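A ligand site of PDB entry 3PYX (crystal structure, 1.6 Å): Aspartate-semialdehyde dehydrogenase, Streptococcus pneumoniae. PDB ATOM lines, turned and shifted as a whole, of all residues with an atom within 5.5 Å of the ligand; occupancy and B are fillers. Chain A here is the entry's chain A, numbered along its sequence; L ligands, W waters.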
ATOM      1  N   VAL A   8      12.160  30.602 -23.741  1.00  0.00           N
ATOM      2  CA  VAL A   8      12.317  29.202 -23.307  1.00  0.00           C
ATOM      3  C   VAL A   8      13.746  29.031 -22.779  1.00  0.00           C
ATOM      4  O   VAL A   8      14.722  29.222 -23.513  1.00  0.00           O
ATOM      5  CB  VAL A   8      12.037  28.236 -24.482  1.00  0.00           C
ATOM      6  CG1 VAL A   8      12.071  26.771 -24.008  1.00  0.00           C
ATOM      7  CG2 VAL A   8      10.657  28.527 -25.099  1.00  0.00           C
ATOM      8  N   GLY A   9      13.849  28.700 -21.492  1.00  0.00           N
ATOM      9  CA  GLY A   9      15.140  28.718 -20.787  1.00  0.00           C
ATOM     10  C   GLY A   9      15.401  30.047 -20.097  1.00  0.00           C
ATOM     11  O   GLY A   9      16.545  30.497 -20.010  1.00  0.00           O
ATOM     12  N   ALA A  10      14.348  30.677 -19.582  1.00  0.00           N
ATOM     13  CA  ALA A  10      14.430  32.028 -18.991  1.00  0.00           C
ATOM     14  C   ALA A  10      15.374  32.140 -17.789  1.00  0.00           C
ATOM     15  O   ALA A  10      15.871  33.219 -17.489  1.00  0.00           O
ATOM     16  CB  ALA A  10      13.013  32.517 -18.616  1.00  0.00           C
ATOM     17  N   THR A  11      15.629  31.014 -17.130  1.00  0.00           N
ATOM     18  CA  THR A  11      16.315  31.000 -15.842  1.00  0.00           C
ATOM     19  C   THR A  11      17.831  30.780 -15.955  1.00  0.00           C
ATOM     20  O   THR A  11      18.567  30.948 -14.960  1.00  0.00           O
ATOM     21  CB  THR A  11      15.725  29.916 -14.911  1.00  0.00           C
ATOM     22  OG1 THR A  11      15.731  28.666 -15.601  1.00  0.00           O
ATOM     23  CG2 THR A  11      14.281  30.248 -14.505  1.00  0.00           C
ATOM     24  N   GLY A  12      18.301  30.439 -17.158  1.00  0.00           N
ATOM     25  CA  GLY A  12      19.728  30.116 -17.373  1.00  0.00           C
ATOM     26  C   GLY A  12      20.613  31.314 -17.683  1.00  0.00           C
ATOM     27  O   GLY A  12      20.179  32.470 -17.603  1.00  0.00           O
ATOM     28  N   ALA A  13      21.884  31.046 -18.030  1.00  0.00           N
ATOM     29  CA  ALA A  13      22.851  32.100 -18.318  1.00  0.00           C
ATOM     30  C   ALA A  13      22.396  32.933 -19.521  1.00  0.00           C
ATOM     31  O   ALA A  13      22.379  34.178 -19.463  1.00  0.00           O
ATOM     32  CB  ALA A  13      24.235  31.501 -18.562  1.00  0.00           C
ATOM     33  N   VAL A  14      22.044  32.250 -20.611  1.00  0.00           N
ATOM     34  CA  VAL A  14      21.570  32.945 -21.806  1.00  0.00           C
ATOM     35  C   VAL A  14      20.193  33.589 -21.534  1.00  0.00           C
ATOM     36  O   VAL A  14      19.971  34.757 -21.897  1.00  0.00           O
ATOM     37  CB  VAL A  14      21.521  32.007 -23.046  1.00  0.00           C
ATOM     38  CG1 VAL A  14      20.839  32.735 -24.222  1.00  0.00           C
ATOM     39  CG2 VAL A  14      22.932  31.550 -23.448  1.00  0.00           C
ATOM     40  N   GLY A  15      19.296  32.821 -20.902  1.00  0.00           N
ATOM     41  CA  GLY A  15      17.938  33.288 -20.578  1.00  0.00           C
ATOM     42  C   GLY A  15      17.923  34.611 -19.843  1.00  0.00           C
ATOM     43  O   GLY A  15      17.122  35.497 -20.197  1.00  0.00           O
ATOM     44  N   LEU A  35       9.384  30.585 -19.859  1.00  0.00           N
ATOM     45  CA  LEU A  35       9.245  29.138 -19.799  1.00  0.00           C
ATOM     46  C   LEU A  35      10.575  28.486 -19.420  1.00  0.00           C
ATOM     47  O   LEU A  35      11.631  28.928 -19.875  1.00  0.00           O
ATOM     48  CB  LEU A  35       8.767  28.577 -21.138  1.00  0.00           C
ATOM     49  CG  LEU A  35       7.274  28.616 -21.475  1.00  0.00           C
ATOM     50  CD1 LEU A  35       6.737  30.027 -21.558  1.00  0.00           C
ATOM     51  CD2 LEU A  35       7.048  27.915 -22.792  1.00  0.00           C
ATOM     52  N   ALA A  36      10.498  27.439 -18.604  1.00  0.00           N
ATOM     53  CA  ALA A  36      11.672  26.661 -18.227  1.00  0.00           C
ATOM     54  C   ALA A  36      11.218  25.229 -17.913  1.00  0.00           C
ATOM     55  O   ALA A  36      10.230  24.752 -18.475  1.00  0.00           O
ATOM     56  CB  ALA A  36      12.395  27.306 -17.032  1.00  0.00           C
ATOM     57  N   SER A  37      11.947  24.530 -17.034  1.00  0.00           N
ATOM     58  CA  SER A  37      11.573  23.164 -16.683  1.00  0.00           C
ATOM     59  C   SER A  37      10.569  23.155 -15.530  1.00  0.00           C
ATOM     60  O   SER A  37      10.315  24.185 -14.888  1.00  0.00           O
ATOM     61  CB  SER A  37      12.803  22.343 -16.303  1.00  0.00           C
ATOM     62  OG  SER A  37      13.233  22.652 -14.996  1.00  0.00           O
ATOM     63  N   ALA A  38      10.000  21.973 -15.271  1.00  0.00           N
ATOM     64  CA  ALA A  38       9.010  21.784 -14.201  1.00  0.00           C
ATOM     65  C   ALA A  38       9.480  22.327 -12.838  1.00  0.00           C
ATOM     66  O   ALA A  38       8.675  22.875 -12.088  1.00  0.00           O
ATOM     67  CB  ALA A  38       8.640  20.308 -14.091  1.00  0.00           C
ATOM     68  N   ARG A  39      10.774  22.198 -12.540  1.00  0.00           N
ATOM     69  CA  ARG A  39      11.316  22.654 -11.251  1.00  0.00           C
ATOM     70  C   ARG A  39      11.359  24.177 -11.099  1.00  0.00           C
ATOM     71  O   ARG A  39      11.553  24.679  -9.988  1.00  0.00           O
ATOM     72  CB  ARG A  39      12.701  22.062 -11.001  1.00  0.00           C
ATOM     73  CG  ARG A  39      13.808  22.712 -11.774  1.00  0.00           C
ATOM     74  CD  ARG A  39      15.102  22.019 -11.534  1.00  0.00           C
ATOM     75  NE  ARG A  39      16.136  22.466 -12.464  1.00  0.00           N
ATOM     76  CZ  ARG A  39      17.401  22.072 -12.418  1.00  0.00           C
ATOM     77  NH1 ARG A  39      17.803  21.211 -11.479  1.00  0.00           N
ATOM     78  NH2 ARG A  39      18.263  22.550 -13.305  1.00  0.00           N
ATOM     79  N   SER A  40      11.200  24.905 -12.205  1.00  0.00           N
ATOM     80  CA  SER A  40      11.159  26.359 -12.160  1.00  0.00           C
ATOM     81  C   SER A  40       9.743  26.908 -12.190  1.00  0.00           C
ATOM     82  O   SER A  40       9.515  28.068 -11.820  1.00  0.00           O
ATOM     83  CB  SER A  40      11.951  26.971 -13.318  1.00  0.00           C
ATOM     84  OG  SER A  40      13.345  26.772 -13.146  1.00  0.00           O
ATOM     85  N   THR A  57       7.720  24.174 -19.732  1.00  0.00           N
ATOM     86  CA  THR A  57       7.700  24.006 -21.184  1.00  0.00           C
ATOM     87  C   THR A  57       7.045  22.669 -21.543  1.00  0.00           C
ATOM     88  O   THR A  57       7.484  21.610 -21.079  1.00  0.00           O
ATOM     89  CB  THR A  57       9.127  24.116 -21.794  1.00  0.00           C
ATOM     90  OG1 THR A  57       9.778  25.289 -21.287  1.00  0.00           O
ATOM     91  CG2 THR A  57       9.055  24.205 -23.320  1.00  0.00           C
ATOM     92  N   SER A  71      16.518  28.966 -25.543  1.00  0.00           N
ATOM     93  CA  SER A  71      17.863  28.773 -25.044  1.00  0.00           C
ATOM     94  C   SER A  71      17.840  27.858 -23.832  1.00  0.00           C
ATOM     95  O   SER A  71      18.204  28.247 -22.714  1.00  0.00           O
ATOM     96  CB  SER A  71      18.508  30.100 -24.684  1.00  0.00           C
ATOM     97  OG  SER A  71      19.894  29.847 -24.454  1.00  0.00           O
ATOM     98  N   ALA A  72      17.433  26.621 -24.072  1.00  0.00           N
ATOM     99  CA  ALA A  72      17.194  25.650 -22.998  1.00  0.00           C
ATOM    100  C   ALA A  72      17.834  24.289 -23.255  1.00  0.00           C
ATOM    101  O   ALA A  72      17.412  23.279 -22.673  1.00  0.00           O
ATOM    102  CB  ALA A  72      15.693  25.505 -22.788  1.00  0.00           C
ATOM    103  N   GLY A  73      18.860  24.252 -24.113  1.00  0.00           N
ATOM    104  CA  GLY A  73      19.555  22.997 -24.435  1.00  0.00           C
ATOM    105  C   GLY A  73      18.981  22.351 -25.687  1.00  0.00           C
ATOM    106  O   GLY A  73      17.786  22.450 -25.932  1.00  0.00           O
ATOM    107  N   SER A  74      19.831  21.706 -26.482  1.00  0.00           N
ATOM    108  CA  SER A  74      19.401  21.135 -27.767  1.00  0.00           C
ATOM    109  C   SER A  74      18.222  20.152 -27.667  1.00  0.00           C
ATOM    110  O   SER A  74      17.333  20.135 -28.515  1.00  0.00           O
ATOM    111  CB  SER A  74      20.585  20.493 -28.502  1.00  0.00           C
ATOM    112  OG  SER A  74      20.976  19.308 -27.833  1.00  0.00           O
ATOM    113  N   THR A  76      15.749  20.262 -25.613  1.00  0.00           N
ATOM    114  CA  THR A  76      14.496  20.998 -25.392  1.00  0.00           C
ATOM    115  C   THR A  76      13.992  21.621 -26.699  1.00  0.00           C
ATOM    116  O   THR A  76      12.777  21.700 -26.942  1.00  0.00           O
ATOM    117  CB  THR A  76      14.692  22.066 -24.288  1.00  0.00           C
ATOM    118  OG1 THR A  76      15.097  21.419 -23.076  1.00  0.00           O
ATOM    119  CG2 THR A  76      13.400  22.842 -24.033  1.00  0.00           C
ATOM    120  N   LYS A  79      12.659  18.735 -28.919  1.00  0.00           N
ATOM    121  CA  LYS A  79      11.349  18.324 -28.425  1.00  0.00           C
ATOM    122  C   LYS A  79      10.213  19.315 -28.693  1.00  0.00           C
ATOM    123  O   LYS A  79       9.160  18.918 -29.178  1.00  0.00           O
ATOM    124  CB  LYS A  79      11.410  17.978 -26.936  1.00  0.00           C
ATOM    125  CG  LYS A  79      11.981  16.586 -26.661  1.00  0.00           C
ATOM    126  CD  LYS A  79      11.686  16.111 -25.234  1.00  0.00           C
ATOM    127  CE  LYS A  79      12.932  16.105 -24.349  1.00  0.00           C
ATOM    128  NZ  LYS A  79      13.219  17.432 -23.721  1.00  0.00           N
ATOM    129  N   TYR A  80      10.430  20.610 -28.408  1.00  0.00           N
ATOM    130  CA  TYR A  80       9.320  21.559 -28.387  1.00  0.00           C
ATOM    131  C   TYR A  80       9.244  22.576 -29.536  1.00  0.00           C
ATOM    132  O   TYR A  80       8.143  23.056 -29.860  1.00  0.00           O
ATOM    133  CB  TYR A  80       9.251  22.280 -27.024  1.00  0.00           C
ATOM    134  CG  TYR A  80       9.139  21.315 -25.873  1.00  0.00           C
ATOM    135  CD1 TYR A  80       7.962  20.601 -25.645  1.00  0.00           C
ATOM    136  CD2 TYR A  80      10.226  21.086 -25.016  1.00  0.00           C
ATOM    137  CE1 TYR A  80       7.855  19.707 -24.598  1.00  0.00           C
ATOM    138  CE2 TYR A  80      10.131  20.192 -23.962  1.00  0.00           C
ATOM    139  CZ  TYR A  80       8.942  19.503 -23.767  1.00  0.00           C
ATOM    140  OH  TYR A  80       8.833  18.623 -22.716  1.00  0.00           O
ATOM    141  N   ASN A  94      18.829  29.208 -30.039  1.00  0.00           N
ATOM    142  CA  ASN A  94      20.236  29.358 -29.702  1.00  0.00           C
ATOM    143  C   ASN A  94      21.029  28.056 -29.703  1.00  0.00           C
ATOM    144  O   ASN A  94      22.273  28.083 -29.663  1.00  0.00           O
ATOM    145  CB  ASN A  94      20.434  30.014 -28.322  1.00  0.00           C
ATOM    146  CG  ASN A  94      20.322  31.506 -28.359  1.00  0.00           C
ATOM    147  OD1 ASN A  94      21.187  32.195 -28.923  1.00  0.00           O
ATOM    148  ND2 ASN A  94      19.294  32.027 -27.725  1.00  0.00           N
ATOM    149  N   THR A  95      20.326  26.927 -29.761  1.00  0.00           N
ATOM    150  CA  THR A  95      20.998  25.604 -29.671  1.00  0.00           C
ATOM    151  C   THR A  95      21.630  25.173 -30.995  1.00  0.00           C
ATOM    152  O   THR A  95      21.370  25.759 -32.046  1.00  0.00           O
ATOM    153  CB  THR A  95      20.070  24.479 -29.154  1.00  0.00           C
ATOM    154  OG1 THR A  95      19.270  23.942 -30.227  1.00  0.00           O
ATOM    155  CG2 THR A  95      19.179  24.950 -28.002  1.00  0.00           C
ATOM    156  N   SER A  96      22.422  24.104 -30.941  1.00  0.00           N
ATOM    157  CA  SER A  96      23.063  23.591 -32.142  1.00  0.00           C
ATOM    158  C   SER A  96      22.127  22.685 -32.946  1.00  0.00           C
ATOM    159  O   SER A  96      22.454  22.351 -34.086  1.00  0.00           O
ATOM    160  CB  SER A  96      24.363  22.857 -31.786  1.00  0.00           C
ATOM    161  OG  SER A  96      24.092  21.777 -30.911  1.00  0.00           O
ATOM    162  N   ARG A  99      20.946  23.778 -36.606  1.00  0.00           N
ATOM    163  CA  ARG A  99      21.851  24.659 -37.372  1.00  0.00           C
ATOM    164  C   ARG A  99      22.233  24.195 -38.767  1.00  0.00           C
ATOM    165  O   ARG A  99      22.454  25.008 -39.658  1.00  0.00           O
ATOM    166  CB  ARG A  99      23.138  24.926 -36.594  1.00  0.00           C
ATOM    167  CG  ARG A  99      22.916  25.743 -35.327  1.00  0.00           C
ATOM    168  CD  ARG A  99      24.242  26.205 -34.737  1.00  0.00           C
ATOM    169  NE  ARG A  99      24.039  26.842 -33.433  1.00  0.00           N
ATOM    170  CZ  ARG A  99      24.842  26.709 -32.378  1.00  0.00           C
ATOM    171  NH1 ARG A  99      25.951  25.971 -32.448  1.00  0.00           N
ATOM    172  NH2 ARG A  99      24.536  27.317 -31.239  1.00  0.00           N
ATOM    173  N   PRO A 126      23.930  30.943 -34.670  1.00  0.00           N
ATOM    174  CA  PRO A 126      25.144  30.115 -34.648  1.00  0.00           C
ATOM    175  C   PRO A 126      25.781  30.043 -33.253  1.00  0.00           C
ATOM    176  O   PRO A 126      25.361  30.707 -32.309  1.00  0.00           O
ATOM    177  CB  PRO A 126      26.084  30.822 -35.627  1.00  0.00           C
ATOM    178  CG  PRO A 126      25.238  31.822 -36.390  1.00  0.00           C
ATOM    179  CD  PRO A 126      24.095  32.161 -35.481  1.00  0.00           C
ATOM    180  N   ASN A 127      26.790  29.201 -33.168  1.00  0.00           N
ATOM    181  CA  ASN A 127      27.666  29.109 -32.015  1.00  0.00           C
ATOM    182  C   ASN A 127      28.298  30.472 -31.698  1.00  0.00           C
ATOM    183  O   ASN A 127      28.695  31.205 -32.602  1.00  0.00           O
ATOM    184  CB  ASN A 127      28.719  28.070 -32.426  1.00  0.00           C
ATOM    185  CG  ASN A 127      29.977  28.130 -31.644  1.00  0.00           C
ATOM    186  OD1 ASN A 127      30.960  28.699 -32.110  1.00  0.00           O
ATOM    187  ND2 ASN A 127      29.981  27.518 -30.466  1.00  0.00           N
ATOM    188  N   CYS A 128      28.416  30.783 -30.408  1.00  0.00           N
ATOM    189  CA  CYS A 128      28.960  32.086 -29.999  1.00  0.00           C
ATOM    190  C   CYS A 128      30.318  32.387 -30.623  1.00  0.00           C
ATOM    191  O   CYS A 128      30.559  33.500 -31.132  1.00  0.00           O
ATOM    192  CB  CYS A 128      29.035  32.181 -28.468  1.00  0.00           C
ATOM    193  SG  CYS A 128      29.714  30.704 -27.699  1.00  0.00           S
ATOM    194  N   SER A 158      31.183  31.064 -18.910  1.00  0.00           N
ATOM    195  CA  SER A 158      29.731  31.253 -19.047  1.00  0.00           C
ATOM    196  C   SER A 158      29.160  30.594 -20.303  1.00  0.00           C
ATOM    197  O   SER A 158      27.963  30.343 -20.376  1.00  0.00           O
ATOM    198  CB  SER A 158      29.309  32.720 -18.968  1.00  0.00           C
ATOM    199  OG  SER A 158      29.790  33.436 -20.088  1.00  0.00           O
ATOM    200  N   GLY A 159      30.020  30.319 -21.296  1.00  0.00           N
ATOM    201  CA  GLY A 159      29.625  29.567 -22.491  1.00  0.00           C
ATOM    202  C   GLY A 159      29.066  28.190 -22.157  1.00  0.00           C
ATOM    203  O   GLY A 159      28.315  27.588 -22.951  1.00  0.00           O
ATOM    204  N   ALA A 160      29.423  27.662 -20.981  1.00  0.00           N
ATOM    205  CA  ALA A 160      29.028  26.312 -20.584  1.00  0.00           C
ATOM    206  C   ALA A 160      27.862  26.358 -19.606  1.00  0.00           C
ATOM    207  O   ALA A 160      27.437  25.313 -19.097  1.00  0.00           O
ATOM    208  CB  ALA A 160      30.216  25.557 -19.973  1.00  0.00           C
ATOM    209  N   GLY A 161      27.334  27.554 -19.358  1.00  0.00           N
ATOM    210  CA  GLY A 161      26.129  27.715 -18.545  1.00  0.00           C
ATOM    211  C   GLY A 161      26.359  28.246 -17.142  1.00  0.00           C
ATOM    212  O   GLY A 161      27.483  28.385 -16.689  1.00  0.00           O
ATOM    213  N   MET A 162      25.267  28.531 -16.451  1.00  0.00           N
ATOM    214  CA  MET A 162      25.348  29.043 -15.081  1.00  0.00           C
ATOM    215  C   MET A 162      26.213  28.191 -14.148  1.00  0.00           C
ATOM    216  O   MET A 162      26.961  28.722 -13.313  1.00  0.00           O
ATOM    217  CB  MET A 162      23.943  29.143 -14.505  1.00  0.00           C
ATOM    218  CG  MET A 162      23.824  30.260 -13.526  1.00  0.00           C
ATOM    219  SD  MET A 162      23.864  31.833 -14.409  1.00  0.00           S
ATOM    220  CE  MET A 162      22.098  32.174 -14.538  1.00  0.00           C
ATOM    221  N   GLY A 163      26.080  26.875 -14.267  1.00  0.00           N
ATOM    222  CA  GLY A 163      26.775  25.937 -13.364  1.00  0.00           C
ATOM    223  C   GLY A 163      28.288  26.077 -13.515  1.00  0.00           C
ATOM    224  O   GLY A 163      29.006  26.078 -12.515  1.00  0.00           O
ATOM    225  N   HIS A 252      34.373  35.941 -25.032  1.00  0.00           N
ATOM    226  CA  HIS A 252      35.340  35.090 -25.722  1.00  0.00           C
ATOM    227  C   HIS A 252      36.344  35.926 -26.497  1.00  0.00           C
ATOM    228  O   HIS A 252      36.005  36.941 -27.113  1.00  0.00           O
ATOM    229  CB  HIS A 252      34.654  34.193 -26.759  1.00  0.00           C
ATOM    230  CG  HIS A 252      33.735  33.165 -26.185  1.00  0.00           C
ATOM    231  ND1 HIS A 252      33.777  32.728 -24.876  1.00  0.00           N
ATOM    232  CD2 HIS A 252      32.783  32.404 -26.791  1.00  0.00           C
ATOM    233  CE1 HIS A 252      32.870  31.789 -24.697  1.00  0.00           C
ATOM    234  NE2 HIS A 252      32.251  31.580 -25.843  1.00  0.00           N
ATOM    235  N   ASN A 325      30.090  36.670 -25.057  1.00  0.00           N
ATOM    236  CA  ASN A 325      29.506  35.432 -25.579  1.00  0.00           C
ATOM    237  C   ASN A 325      28.024  35.215 -25.249  1.00  0.00           C
ATOM    238  O   ASN A 325      27.348  34.405 -25.876  1.00  0.00           O
ATOM    239  CB  ASN A 325      30.326  34.243 -25.066  1.00  0.00           C
ATOM    240  CG  ASN A 325      30.368  34.184 -23.533  1.00  0.00           C
ATOM    241  OD1 ASN A 325      30.982  35.036 -22.887  1.00  0.00           O
ATOM    242  ND2 ASN A 325      29.696  33.215 -22.956  1.00  0.00           N
ATOM    243  N   LEU A 326      27.520  35.938 -24.240  1.00  0.00           N
ATOM    244  CA  LEU A 326      26.087  35.851 -23.900  1.00  0.00           C
ATOM    245  C   LEU A 326      25.279  36.916 -24.628  1.00  0.00           C
ATOM    246  O   LEU A 326      24.051  36.816 -24.670  1.00  0.00           O
ATOM    247  CB  LEU A 326      25.878  35.978 -22.389  1.00  0.00           C
ATOM    248  CG  LEU A 326      26.528  34.892 -21.528  1.00  0.00           C
ATOM    249  CD1 LEU A 326      26.150  35.048 -20.067  1.00  0.00           C
ATOM    250  CD2 LEU A 326      26.124  33.525 -22.034  1.00  0.00           C
ATOM    251  N   GLY A 329      27.195  36.762 -28.851  1.00  0.00           N
ATOM    252  CA  GLY A 329      27.309  35.307 -28.991  1.00  0.00           C
ATOM    253  C   GLY A 329      26.038  34.505 -28.768  1.00  0.00           C
ATOM    254  O   GLY A 329      25.982  33.321 -29.135  1.00  0.00           O
ATOM    255  N   ALA A 330      24.993  35.113 -28.192  1.00  0.00           N
ATOM    256  CA  ALA A 330      23.749  34.376 -27.942  1.00  0.00           C
ATOM    257  C   ALA A 330      22.521  35.295 -27.887  1.00  0.00           C
ATOM    258  O   ALA A 330      21.812  35.424 -28.879  1.00  0.00           O
ATOM    259  CB  ALA A 330      23.870  33.530 -26.647  1.00  0.00           C
HETATM  260  P1  LIG L   1      22.173  27.103 -18.424  1.00  0.00           P
HETATM  261  O1  LIG L   1      22.566  25.800 -17.828  1.00  0.00           O
HETATM  262  O2  LIG L   1      22.672  28.307 -17.714  1.00  0.00           O
HETATM  263  O3  LIG L   1      20.559  27.158 -18.440  1.00  0.00           O
HETATM  264  C1  LIG L   1      19.797  26.059 -18.879  1.00  0.00           C
HETATM  265  C2  LIG L   1      18.360  26.558 -19.096  1.00  0.00           C
HETATM  266  O4  LIG L   1      17.652  25.538 -19.776  1.00  0.00           O
HETATM  267  C3  LIG L   1      17.606  26.836 -17.804  1.00  0.00           C
HETATM  268  O5  LIG L   1      16.679  27.890 -17.999  1.00  0.00           O
HETATM  269  C4  LIG L   1      16.839  25.533 -17.600  1.00  0.00           C
HETATM  270  O6  LIG L   1      15.690  25.687 -16.818  1.00  0.00           O
HETATM  271  C5  LIG L   1      16.481  25.227 -19.040  1.00  0.00           C
HETATM  272  N1  LIG L   1      16.045  23.841 -19.207  1.00  0.00           N
HETATM  273  C6  LIG L   1      16.762  22.688 -18.970  1.00  0.00           C
HETATM  274  N2  LIG L   1      15.958  21.638 -19.255  1.00  0.00           N
HETATM  275  C7  LIG L   1      14.751  22.092 -19.653  1.00  0.00           C
HETATM  276  C8  LIG L   1      13.586  21.461 -20.048  1.00  0.00           C
HETATM  277  N3  LIG L   1      13.541  20.139 -20.083  1.00  0.00           N
HETATM  278  N4  LIG L   1      12.488  22.218 -20.411  1.00  0.00           N
HETATM  279  C9  LIG L   1      12.550  23.601 -20.386  1.00  0.00           C
HETATM  280  N5  LIG L   1      13.710  24.228 -19.983  1.00  0.00           N
HETATM  281  C10 LIG L   1      14.787  23.491 -19.625  1.00  0.00           C
HETATM  282  O7  LIG L   1      22.552  27.100 -20.004  1.00  0.00           O
HETATM  283  P2  LIG L   1      22.914  28.300 -21.045  1.00  0.00           P
HETATM  284  O8  LIG L   1      24.372  28.607 -21.054  1.00  0.00           O
HETATM  285  O9  LIG L   1      21.981  29.430 -20.808  1.00  0.00           O
HETATM  286  O10 LIG L   1      22.638  27.597 -22.464  1.00  0.00           O
HETATM  287  C11 LIG L   1      21.351  27.366 -23.011  1.00  0.00           C
HETATM  288  C12 LIG L   1      21.472  27.002 -24.495  1.00  0.00           C
HETATM  289  O11 LIG L   1      22.057  28.065 -25.228  1.00  0.00           O
HETATM  290  C13 LIG L   1      22.349  25.777 -24.755  1.00  0.00           C
HETATM  291  O12 LIG L   1      21.720  25.061 -25.789  1.00  0.00           O
HETATM  292  C14 LIG L   1      23.643  26.355 -25.291  1.00  0.00           C
HETATM  293  O13 LIG L   1      24.343  25.499 -26.182  1.00  0.00           O
HETATM  294  C15 LIG L   1      23.161  27.612 -25.999  1.00  0.00           C
HETATM  295  N6  LIG L   1      24.200  28.648 -26.115  1.00  0.00           N
HETATM  296  C16 LIG L   1      24.902  29.058 -25.005  1.00  0.00           C
HETATM  297  C17 LIG L   1      25.876  30.036 -25.130  1.00  0.00           C
HETATM  298  C18 LIG L   1      26.551  30.628 -23.943  1.00  0.00           C
HETATM  299  O14 LIG L   1      27.598  31.551 -24.205  1.00  0.00           O
HETATM  300  N7  LIG L   1      26.149  30.262 -22.705  1.00  0.00           N
HETATM  301  C19 LIG L   1      26.131  30.599 -26.379  1.00  0.00           C
HETATM  302  C20 LIG L   1      25.415  30.173 -27.495  1.00  0.00           C
HETATM  303  C21 LIG L   1      24.454  29.185 -27.339  1.00  0.00           C
HETATM  304  P3  LIG L   1      15.654  25.286 -15.239  1.00  0.00           P
HETATM  305  O15 LIG L   1      14.189  25.130 -14.918  1.00  0.00           O
HETATM  306  O16 LIG L   1      16.406  23.997 -15.050  1.00  0.00           O
HETATM  307  O17 LIG L   1      16.283  26.424 -14.447  1.00  0.00           O
HETATM  308  O   HOH W   1      25.834  26.780 -22.310  1.00  0.00           O
HETATM  309  O   HOH W   2      23.475  23.717 -28.165  1.00  0.00           O
HETATM  310  O   HOH W   3      19.453  30.000 -20.563  1.00  0.00           O
HETATM  311  O   HOH W   4      19.197  26.246 -14.471  1.00  0.00           O
HETATM  312  O   HOH W   5      11.070  18.437 -20.829  1.00  0.00           O
HETATM  313  O   HOH W   6      16.177  21.344 -15.829  1.00  0.00           O
HETATM  314  O   HOH W   7      10.105  21.404 -19.599  1.00  0.00           O
HETATM  315  O   HOH W   8      24.004  31.598 -30.160  1.00  0.00           O
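Water W3 lies within hydrogen-bond range of O9 of the ligand (2.6 Å), N of Gly 15 (2.8 Å), O of Gly 9 (3.0 Å), O of Ser 71 (3.0 Å) and N of Val 14 (3.4 Å). Water W7 bridges a nitrogen (N4) of the ligand (2.6 Å) and the backbone carbonyl oxygen (O) of Thr 57 (3.0 Å). Water W1 lies within hydrogen-bond range of O8 of the ligand, O of Gly 159 and N of Gly 161. Water W6 lies within hydrogen-bond range of an oxygen (O16) of the ligand (2.8 Å), the side-chain hydroxyl (OG) of Ser 37 (3.3 Å) and the guanidinium group (NH2) of Arg 39 (3.5 Å). Water W2 bridges an oxygen (O13) of the ligand (2.8 Å) and the backbone NH (N) of Ser 96 (3.0 Å). Water W5 lies within hydrogen-bond range of the side-chain hydroxyl (OH) of Tyr 80 (2.9 Å) and a nitrogen (N3) of the ligand (3.1 Å).
The side-chain hydroxyl of Ser 158 is in hydrogen-bond range of the side-chain amide nitrogen of Asn 325 (2.9 Å). The guanidinium group (NE) of Arg 99 sits at hydrogen-bond distance from the backbone carbonyl oxygen (O) of Thr 95 (3.2 Å). The backbone NH (N) of Ala 10 lies within hydrogen-bond range of the backbone carbonyl oxygen (O) of Leu 35, at 3.2 Å. The backbone carbonyl oxygen (O) of Asn 94 is in hydrogen-bond range of the guanidinium group (NH2) of Arg 99, at 2.9 Å. The backbone NH (N) of Gly 159 lies close to the side-chain amide nitrogen (ND2) of Asn 325 (3.4 Å). O of Ala 72 lies within hydrogen-bond range of OG1 of Thr 76 (3.0 Å). O of Val 8 is in hydrogen-bond range of N of Ser 71 (2.7 Å). The backbone carbonyl oxygen of Ala 36 sits at hydrogen-bond distance from the backbone NH of Thr 57.
Residues that only touch the ligand: Gly 161, Ala 36, Ala 72, Leu 326, Thr 57, Thr 95, Asn 94, Thr 76, Gly 329, Ala 330, Cys 128, Ser 74 and Ala 10. Within 4 Å of the ligand: Gly 9, Ala 10, Thr 11, Gly 12, Ala 13, Val 14, Ala 36, Ser 37, Arg 39, Ser 40, Thr 57, Ser 71, Ala 72, Gly 73, Ser 74, Thr 76, Asn 94, Thr 95, Cys 128, Ser 158, Gly 159, Gly 161, Met 162, Asn 325, Leu 326, Gly 329 and Ala 330. The nearest printed residue that does not touch the ligand is Arg 99 (4.3 Å).
The backbone carbonyl oxygen (O) of Gly 9 lies close to an oxygen (O5) of the ligand (3.3 Å). The backbone NH of Met 162 is in hydrogen-bond range of an oxygen (O2) of the ligand (2.9 Å). N of Gly 73 sits close to O12 of the ligand, at 3.4 Å. The side-chain hydroxyl (OG) of Ser 71 sits at hydrogen-bond distance from an oxygen (O11) of the ligand. A nitrogen (N7) of the ligand lies within hydrogen-bond range of the backbone carbonyl oxygen (O) of Ser 158, 3.0 Å away. The backbone carbonyl oxygen of Gly 159 is in hydrogen-bond range of a nitrogen (N7) of the ligand, at 3.4 Å. An oxygen (O15) of the ligand lies within hydrogen-bond range of the side-chain hydroxyl (OG) of Ser 40 (2.6 Å). The backbone NH (N) of Gly 12 is in hydrogen-bond range of an oxygen (O5) of the ligand, 3.1 Å away. An oxygen (O17) of the ligand is in hydrogen-bond range of the side-chain hydroxyl of Thr 11, at 2.6 Å. N of Thr 11 lies within hydrogen-bond range of O5 of the ligand (3.4 Å). An oxygen (O15) of the ligand sits at hydrogen-bond distance from the side-chain hydroxyl (OG) of Ser 37. O16 of the ligand lies within salt-bridge range of NH2 of Arg 39 (2.9 Å). An oxygen (O2) of the ligand lies within hydrogen-bond range of the backbone NH (N) of Ala 13, at 2.9 Å. The backbone NH (N) of Ser 37 is in hydrogen-bond range of an oxygen (O15) of the ligand (3.1 Å). ND2 of Asn 325 sits at hydrogen-bond distance from O14 of the ligand (3.0 Å). O9 of the ligand sits at hydrogen-bond distance from N of Val 14 (2.8 Å).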
